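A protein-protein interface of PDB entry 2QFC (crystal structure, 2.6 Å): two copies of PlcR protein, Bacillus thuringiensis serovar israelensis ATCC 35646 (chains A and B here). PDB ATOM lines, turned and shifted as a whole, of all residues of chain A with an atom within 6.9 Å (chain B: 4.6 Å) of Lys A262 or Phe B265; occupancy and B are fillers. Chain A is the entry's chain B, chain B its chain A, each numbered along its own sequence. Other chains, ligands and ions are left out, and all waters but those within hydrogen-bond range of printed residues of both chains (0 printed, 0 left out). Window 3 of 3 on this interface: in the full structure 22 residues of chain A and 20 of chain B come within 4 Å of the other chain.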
ATOM      1  N   ILE A 235       6.208   6.353  24.248  1.00  0.00           N
ATOM      2  CA  ILE A 235       7.366   6.410  23.347  1.00  0.00           C
ATOM      3  C   ILE A 235       7.185   5.741  21.987  1.00  0.00           C
ATOM      4  O   ILE A 235       7.766   6.182  21.001  1.00  0.00           O
ATOM      5  CB  ILE A 235       8.653   5.930  24.030  1.00  0.00           C
ATOM      6  CG1 ILE A 235       9.850   6.659  23.441  1.00  0.00           C
ATOM      7  CG2 ILE A 235       8.789   4.436  23.961  1.00  0.00           C
ATOM      8  CD1 ILE A 235      11.207   6.109  23.919  1.00  0.00           C
ATOM      9  N   GLY A 236       6.385   4.685  21.924  1.00  0.00           N
ATOM     10  CA  GLY A 236       6.068   4.060  20.639  1.00  0.00           C
ATOM     11  C   GLY A 236       5.298   5.072  19.803  1.00  0.00           C
ATOM     12  O   GLY A 236       5.609   5.320  18.628  1.00  0.00           O
ATOM     13  N   TYR A 239       7.819   7.729  18.404  1.00  0.00           N
ATOM     14  CA  TYR A 239       8.650   7.371  17.259  1.00  0.00           C
ATOM     15  C   TYR A 239       7.822   7.331  15.994  1.00  0.00           C
ATOM     16  O   TYR A 239       8.282   7.734  14.900  1.00  0.00           O
ATOM     17  CB  TYR A 239       9.385   6.052  17.495  1.00  0.00           C
ATOM     18  CG  TYR A 239      10.633   6.205  18.337  1.00  0.00           C
ATOM     19  CD1 TYR A 239      11.727   6.956  17.878  1.00  0.00           C
ATOM     20  CD2 TYR A 239      10.741   5.573  19.574  1.00  0.00           C
ATOM     21  CE1 TYR A 239      12.884   7.106  18.643  1.00  0.00           C
ATOM     22  CE2 TYR A 239      11.890   5.717  20.360  1.00  0.00           C
ATOM     23  CZ  TYR A 239      12.950   6.486  19.878  1.00  0.00           C
ATOM     24  OH  TYR A 239      14.087   6.597  20.636  1.00  0.00           O
ATOM     25  N   TYR A 240       6.589   6.880  16.154  1.00  0.00           N
ATOM     26  CA  TYR A 240       5.619   6.821  15.058  1.00  0.00           C
ATOM     27  C   TYR A 240       5.386   8.198  14.499  1.00  0.00           C
ATOM     28  O   TYR A 240       5.462   8.432  13.290  1.00  0.00           O
ATOM     29  CB  TYR A 240       4.284   6.333  15.595  1.00  0.00           C
ATOM     30  CG  TYR A 240       3.241   6.235  14.537  1.00  0.00           C
ATOM     31  CD1 TYR A 240       3.138   5.088  13.763  1.00  0.00           C
ATOM     32  CD2 TYR A 240       2.389   7.298  14.271  1.00  0.00           C
ATOM     33  CE1 TYR A 240       2.210   4.999  12.769  1.00  0.00           C
ATOM     34  CE2 TYR A 240       1.468   7.213  13.301  1.00  0.00           C
ATOM     35  CZ  TYR A 240       1.381   6.059  12.548  1.00  0.00           C
ATOM     36  OH  TYR A 240       0.451   5.950  11.555  1.00  0.00           O
ATOM     37  N   ARG A 242       7.290  10.739  14.923  1.00  0.00           N
ATOM     38  CA  ARG A 242       8.535  11.172  14.355  1.00  0.00           C
ATOM     39  C   ARG A 242       8.592  10.742  12.882  1.00  0.00           C
ATOM     40  O   ARG A 242       8.957  11.529  12.014  1.00  0.00           O
ATOM     41  CB  ARG A 242       9.710  10.606  15.157  1.00  0.00           C
ATOM     42  CG  ARG A 242      11.020  11.324  14.872  1.00  0.00           C
ATOM     43  CD  ARG A 242      12.225  10.809  15.677  1.00  0.00           C
ATOM     44  NE  ARG A 242      13.400  10.690  14.836  1.00  0.00           N
ATOM     45  CZ  ARG A 242      14.200  11.692  14.459  1.00  0.00           C
ATOM     46  NH1 ARG A 242      13.966  12.927  14.863  1.00  0.00           N
ATOM     47  NH2 ARG A 242      15.260  11.446  13.682  1.00  0.00           N
ATOM     48  N   GLU A 257      12.354   5.110   8.048  1.00  0.00           N
ATOM     49  CA  GLU A 257      12.068   3.720   8.353  1.00  0.00           C
ATOM     50  C   GLU A 257      12.623   3.399   9.714  1.00  0.00           C
ATOM     51  O   GLU A 257      12.075   2.555  10.416  1.00  0.00           O
ATOM     52  CB  GLU A 257      12.612   2.768   7.274  1.00  0.00           C
ATOM     53  CG  GLU A 257      13.935   2.094   7.650  1.00  0.00           C
ATOM     54  CD  GLU A 257      14.306   0.953   6.722  1.00  0.00           C
ATOM     55  OE1 GLU A 257      13.511   0.637   5.800  1.00  0.00           O
ATOM     56  OE2 GLU A 257      15.396   0.368   6.911  1.00  0.00           O
ATOM     57  N   ASP A 258      13.687   4.094  10.096  1.00  0.00           N
ATOM     58  CA  ASP A 258      14.280   3.893  11.413  1.00  0.00           C
ATOM     59  C   ASP A 258      13.299   4.266  12.533  1.00  0.00           C
ATOM     60  O   ASP A 258      13.051   3.468  13.441  1.00  0.00           O
ATOM     61  CB  ASP A 258      15.575   4.686  11.549  1.00  0.00           C
ATOM     62  CG  ASP A 258      16.391   4.245  12.731  1.00  0.00           C
ATOM     63  OD1 ASP A 258      16.777   3.051  12.762  1.00  0.00           O
ATOM     64  OD2 ASP A 258      16.641   5.075  13.639  1.00  0.00           O
ATOM     65  N   ALA A 259      12.724   5.463  12.444  1.00  0.00           N
ATOM     66  CA  ALA A 259      11.718   5.889  13.392  1.00  0.00           C
ATOM     67  C   ALA A 259      10.590   4.863  13.503  1.00  0.00           C
ATOM     68  O   ALA A 259      10.188   4.517  14.615  1.00  0.00           O
ATOM     69  CB  ALA A 259      11.178   7.296  13.056  1.00  0.00           C
ATOM     70  N   TYR A 260      10.113   4.359  12.365  1.00  0.00           N
ATOM     71  CA  TYR A 260       8.993   3.409  12.340  1.00  0.00           C
ATOM     72  C   TYR A 260       9.431   2.037  12.850  1.00  0.00           C
ATOM     73  O   TYR A 260       8.660   1.327  13.499  1.00  0.00           O
ATOM     74  CB  TYR A 260       8.421   3.264  10.923  1.00  0.00           C
ATOM     75  CG  TYR A 260       7.601   4.430  10.378  1.00  0.00           C
ATOM     76  CD1 TYR A 260       7.919   5.023   9.163  1.00  0.00           C
ATOM     77  CD2 TYR A 260       6.490   4.889  11.039  1.00  0.00           C
ATOM     78  CE1 TYR A 260       7.145   6.084   8.625  1.00  0.00           C
ATOM     79  CE2 TYR A 260       5.721   5.955  10.543  1.00  0.00           C
ATOM     80  CZ  TYR A 260       6.049   6.545   9.332  1.00  0.00           C
ATOM     81  OH  TYR A 260       5.269   7.581   8.841  1.00  0.00           O
ATOM     82  N   LYS A 261      10.671   1.661  12.555  1.00  0.00           N
ATOM     83  CA  LYS A 261      11.265   0.465  13.175  1.00  0.00           C
ATOM     84  C   LYS A 261      11.207   0.547  14.737  1.00  0.00           C
ATOM     85  O   LYS A 261      10.828  -0.413  15.420  1.00  0.00           O
ATOM     86  CB  LYS A 261      12.728   0.306  12.767  1.00  0.00           C
ATOM     87  CG  LYS A 261      13.056  -0.363  11.445  1.00  0.00           C
ATOM     88  CD  LYS A 261      14.562  -0.760  11.484  1.00  0.00           C
ATOM     89  CE  LYS A 261      15.360  -0.227  10.267  1.00  0.00           C
ATOM     90  NZ  LYS A 261      15.710  -1.269   9.238  1.00  0.00           N
ATOM     91  N   LYS A 262      11.592   1.698  15.282  1.00  0.00           N
ATOM     92  CA  LYS A 262      11.625   1.872  16.721  1.00  0.00           C
ATOM     93  C   LYS A 262      10.201   1.725  17.236  1.00  0.00           C
ATOM     94  O   LYS A 262       9.899   0.859  18.076  1.00  0.00           O
ATOM     95  CB  LYS A 262      12.151   3.251  17.102  1.00  0.00           C
ATOM     96  CG  LYS A 262      13.352   3.729  16.368  1.00  0.00           C
ATOM     97  CD  LYS A 262      14.611   3.241  16.989  1.00  0.00           C
ATOM     98  CE  LYS A 262      15.828   3.801  16.235  1.00  0.00           C
ATOM     99  NZ  LYS A 262      16.339   5.118  16.726  1.00  0.00           N
ATOM    100  N   ALA A 263       9.322   2.548  16.703  1.00  0.00           N
ATOM    101  CA  ALA A 263       7.936   2.470  17.024  1.00  0.00           C
ATOM    102  C   ALA A 263       7.457   1.044  16.971  1.00  0.00           C
ATOM    103  O   ALA A 263       6.771   0.586  17.880  1.00  0.00           O
ATOM    104  CB  ALA A 263       7.149   3.313  16.059  1.00  0.00           C
ATOM    105  N   SER A 264       7.814   0.330  15.904  1.00  0.00           N
ATOM    106  CA  SER A 264       7.321  -1.024  15.753  1.00  0.00           C
ATOM    107  C   SER A 264       7.750  -1.838  16.959  1.00  0.00           C
ATOM    108  O   SER A 264       6.914  -2.406  17.680  1.00  0.00           O
ATOM    109  CB  SER A 264       7.773  -1.672  14.433  1.00  0.00           C
ATOM    110  OG  SER A 264       7.032  -2.869  14.215  1.00  0.00           O
ATOM    111  N   PHE A 265       9.049  -1.832  17.213  1.00  0.00           N
ATOM    112  CA  PHE A 265       9.603  -2.502  18.378  1.00  0.00           C
ATOM    113  C   PHE A 265       8.820  -2.198  19.670  1.00  0.00           C
ATOM    114  O   PHE A 265       8.476  -3.126  20.416  1.00  0.00           O
ATOM    115  CB  PHE A 265      11.049  -2.104  18.514  1.00  0.00           C
ATOM    116  CG  PHE A 265      11.693  -2.585  19.747  1.00  0.00           C
ATOM    117  CD1 PHE A 265      11.978  -3.920  19.915  1.00  0.00           C
ATOM    118  CD2 PHE A 265      12.064  -1.677  20.748  1.00  0.00           C
ATOM    119  CE1 PHE A 265      12.634  -4.383  21.079  1.00  0.00           C
ATOM    120  CE2 PHE A 265      12.715  -2.098  21.892  1.00  0.00           C
ATOM    121  CZ  PHE A 265      13.004  -3.459  22.074  1.00  0.00           C
ATOM    122  N   PHE A 266       8.535  -0.920  19.939  1.00  0.00           N
ATOM    123  CA  PHE A 266       7.778  -0.607  21.147  1.00  0.00           C
ATOM    124  C   PHE A 266       6.389  -1.206  21.120  1.00  0.00           C
ATOM    125  O   PHE A 266       5.873  -1.630  22.147  1.00  0.00           O
ATOM    126  CB  PHE A 266       7.781   0.878  21.494  1.00  0.00           C
ATOM    127  CG  PHE A 266       9.070   1.322  22.115  1.00  0.00           C
ATOM    128  CD1 PHE A 266       9.426   0.888  23.396  1.00  0.00           C
ATOM    129  CD2 PHE A 266       9.971   2.104  21.400  1.00  0.00           C
ATOM    130  CE1 PHE A 266      10.652   1.258  23.964  1.00  0.00           C
ATOM    131  CE2 PHE A 266      11.187   2.484  21.965  1.00  0.00           C
ATOM    132  CZ  PHE A 266      11.534   2.060  23.243  1.00  0.00           C
ATOM    133  N   PHE A 267       5.827  -1.355  19.934  1.00  0.00           N
ATOM    134  CA  PHE A 267       4.489  -1.893  19.858  1.00  0.00           C
ATOM    135  C   PHE A 267       4.356  -3.393  20.144  1.00  0.00           C
ATOM    136  O   PHE A 267       3.325  -3.779  20.709  1.00  0.00           O
ATOM    137  CB  PHE A 267       3.818  -1.491  18.544  1.00  0.00           C
ATOM    138  CG  PHE A 267       3.532  -0.025  18.446  1.00  0.00           C
ATOM    139  CD1 PHE A 267       3.392   0.744  19.592  1.00  0.00           C
ATOM    140  CD2 PHE A 267       3.400   0.591  17.202  1.00  0.00           C
ATOM    141  CE1 PHE A 267       3.142   2.090  19.500  1.00  0.00           C
ATOM    142  CE2 PHE A 267       3.114   1.962  17.107  1.00  0.00           C
ATOM    143  CZ  PHE A 267       2.984   2.701  18.235  1.00  0.00           C
ATOM    144  N   LYS B 261      21.734  -6.580  21.051  1.00  0.00           N
ATOM    145  CA  LYS B 261      21.354  -5.341  20.346  1.00  0.00           C
ATOM    146  C   LYS B 261      20.259  -4.562  21.131  1.00  0.00           C
ATOM    147  O   LYS B 261      20.258  -3.330  21.179  1.00  0.00           O
ATOM    148  CB  LYS B 261      20.833  -5.572  18.917  1.00  0.00           C
ATOM    149  CG  LYS B 261      21.423  -6.690  18.062  1.00  0.00           C
ATOM    150  CD  LYS B 261      20.522  -6.801  16.789  1.00  0.00           C
ATOM    151  CE  LYS B 261      20.820  -8.022  15.878  1.00  0.00           C
ATOM    152  NZ  LYS B 261      21.847  -7.754  14.824  1.00  0.00           N
ATOM    153  N   LYS B 262      19.321  -5.290  21.729  1.00  0.00           N
ATOM    154  CA  LYS B 262      18.244  -4.664  22.452  1.00  0.00           C
ATOM    155  C   LYS B 262      18.795  -3.990  23.679  1.00  0.00           C
ATOM    156  O   LYS B 262      18.613  -2.797  23.863  1.00  0.00           O
ATOM    157  CB  LYS B 262      17.168  -5.673  22.792  1.00  0.00           C
ATOM    158  CG  LYS B 262      16.276  -5.958  21.619  1.00  0.00           C
ATOM    159  CD  LYS B 262      15.511  -7.249  21.786  1.00  0.00           C
ATOM    160  CE  LYS B 262      14.497  -7.426  20.660  1.00  0.00           C
ATOM    161  NZ  LYS B 262      13.375  -8.287  21.111  1.00  0.00           N
ATOM    162  N   ALA B 263      19.517  -4.710  24.502  1.00  0.00           N
ATOM    163  CA  ALA B 263      20.265  -4.031  25.524  1.00  0.00           C
ATOM    164  C   ALA B 263      20.977  -2.803  24.972  1.00  0.00           C
ATOM    165  O   ALA B 263      20.937  -1.727  25.572  1.00  0.00           O
ATOM    166  CB  ALA B 263      21.269  -4.975  26.198  1.00  0.00           C
ATOM    167  N   SER B 264      21.618  -2.947  23.821  1.00  0.00           N
ATOM    168  CA  SER B 264      22.400  -1.850  23.278  1.00  0.00           C
ATOM    169  C   SER B 264      21.470  -0.680  22.959  1.00  0.00           C
ATOM    170  O   SER B 264      21.684   0.446  23.394  1.00  0.00           O
ATOM    171  CB  SER B 264      23.240  -2.318  22.067  1.00  0.00           C
ATOM    172  OG  SER B 264      24.111  -1.298  21.616  1.00  0.00           O
ATOM    173  N   PHE B 265      20.384  -0.967  22.273  1.00  0.00           N
ATOM    174  CA  PHE B 265      19.397   0.058  21.988  1.00  0.00           C
ATOM    175  C   PHE B 265      19.024   0.862  23.246  1.00  0.00           C
ATOM    176  O   PHE B 265      19.030   2.107  23.208  1.00  0.00           O
ATOM    177  CB  PHE B 265      18.181  -0.593  21.374  1.00  0.00           C
ATOM    178  CG  PHE B 265      17.056   0.339  21.110  1.00  0.00           C
ATOM    179  CD1 PHE B 265      17.151   1.286  20.126  1.00  0.00           C
ATOM    180  CD2 PHE B 265      15.850   0.238  21.852  1.00  0.00           C
ATOM    181  CE1 PHE B 265      16.082   2.132  19.859  1.00  0.00           C
ATOM    182  CE2 PHE B 265      14.775   1.061  21.588  1.00  0.00           C
ATOM    183  CZ  PHE B 265      14.882   2.017  20.592  1.00  0.00           C
ATOM    184  N   PHE B 266      18.712   0.171  24.348  1.00  0.00           N
ATOM    185  CA  PHE B 266      18.310   0.904  25.539  1.00  0.00           C
ATOM    186  C   PHE B 266      19.457   1.709  26.093  1.00  0.00           C
ATOM    187  O   PHE B 266      19.241   2.847  26.563  1.00  0.00           O
ATOM    188  CB  PHE B 266      17.620   0.045  26.605  1.00  0.00           C
ATOM    189  CG  PHE B 266      16.256  -0.375  26.197  1.00  0.00           C
ATOM    190  CD1 PHE B 266      15.216   0.574  26.119  1.00  0.00           C
ATOM    191  CD2 PHE B 266      16.013  -1.679  25.788  1.00  0.00           C
ATOM    192  CE1 PHE B 266      13.930   0.197  25.682  1.00  0.00           C
ATOM    193  CE2 PHE B 266      14.749  -2.069  25.361  1.00  0.00           C
ATOM    194  CZ  PHE B 266      13.702  -1.144  25.293  1.00  0.00           C
ATOM    195  N   PHE B 267      20.672   1.189  25.950  1.00  0.00           N
ATOM    196  CA  PHE B 267      21.785   1.903  26.520  1.00  0.00           C
ATOM    197  C   PHE B 267      21.990   3.250  25.869  1.00  0.00           C
ATOM    198  O   PHE B 267      22.114   4.245  26.595  1.00  0.00           O
ATOM    199  CB  PHE B 267      23.069   1.054  26.579  1.00  0.00           C
ATOM    200  CG  PHE B 267      22.961  -0.098  27.532  1.00  0.00           C
ATOM    201  CD1 PHE B 267      22.054  -0.050  28.585  1.00  0.00           C
ATOM    202  CD2 PHE B 267      23.732  -1.231  27.370  1.00  0.00           C
ATOM    203  CE1 PHE B 267      21.917  -1.095  29.443  1.00  0.00           C
ATOM    204  CE2 PHE B 267      23.630  -2.281  28.255  1.00  0.00           C
ATOM    205  CZ  PHE B 267      22.726  -2.223  29.287  1.00  0.00           C
ATOM    206  N   ASP B 268      21.997   3.278  24.529  1.00  0.00           N
ATOM    207  CA  ASP B 268      22.083   4.532  23.750  1.00  0.00           C
ATOM    208  C   ASP B 268      20.884   5.444  23.988  1.00  0.00           C
ATOM    209  O   ASP B 268      21.046   6.598  24.365  1.00  0.00           O
ATOM    210  CB  ASP B 268      22.251   4.263  22.242  1.00  0.00           C
ATOM    211  CG  ASP B 268      23.543   3.504  21.914  1.00  0.00           C
ATOM    212  OD1 ASP B 268      24.468   3.466  22.769  1.00  0.00           O
ATOM    213  OD2 ASP B 268      23.645   2.935  20.798  1.00  0.00           O
ATOM    214  N   ILE B 269      19.688   4.915  23.755  1.00  0.00           N
ATOM    215  CA  ILE B 269      18.414   5.617  24.041  1.00  0.00           C
ATOM    216  C   ILE B 269      18.475   6.255  25.430  1.00  0.00           C
ATOM    217  O   ILE B 269      18.155   7.433  25.576  1.00  0.00           O
ATOM    218  CB  ILE B 269      17.186   4.639  23.820  1.00  0.00           C
ATOM    219  CG1 ILE B 269      16.748   4.688  22.372  1.00  0.00           C
ATOM    220  CG2 ILE B 269      16.004   4.902  24.663  1.00  0.00           C
ATOM    221  CD1 ILE B 269      17.201   5.886  21.681  1.00  0.00           C
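Printed residues of chain A that touch a printed residue of chain B: Tyr A239, Lys A262, Phe A265 and Phe A266. Hydrophobic or aromatic side chains of chain A that line the printed part of chain B: Tyr A239, Phe A265 and Phe A266.
Lys A262 touches Phe B265, and with the chains exchanged Phe A265 touches Lys B262. Phe A265 touches its own counterpart, Phe B265. Phe A265 touches Phe B266, and with the chains exchanged Phe A266 touches Phe B265. Phe B266 touches its own counterpart, Phe A266. Positions printed for both chains: 261, 262, 263, 264, 265, 266 and 267. Of the 7 pairs that touch across the chains among the printed residues, 6 have their exchanged pair printed and touching as well.
The side-chain carboxylate (OD2) of Asp A258 lies within salt-bridge range of the side-chain amino group (NZ) of Lys A262, 3.1 Å away.
Among the printed residues, pairs that only touch across the chains: Tyr A239 with Ile B269, Lys A262 with Phe B265, Phe A265 with Lys B262, Phe A265 with Phe B266, Phe A266 with Phe B265, Phe A265 with Phe B265 and Phe A266 with Phe B266.
Of the printed residues of chain B, Tyr A239 touches Ile B269. Ala A259 touches none of the printed residues of chain B. Of chain B, only Phe B265 comes within 4 Å of Lys A262. Of the printed residues of chain B, Phe A265 touches Lys B262 (3.6 Å), Phe B265 (3.8 Å) and Phe B266 (3.7 Å). Phe A267 touches none of the printed residues of chain B. Printed residues of chain A within 4 Å of Lys B262: Phe A265 (3.6 Å). Printed residues of chain A within 4 Å of Phe B265: Lys A262 (3.4 Å), Phe A265 (3.8 Å) and Phe A266 (3.8 Å). The nearest residue of chain A that does not touch Phe B265 is Tyr A239 (4.6 Å).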
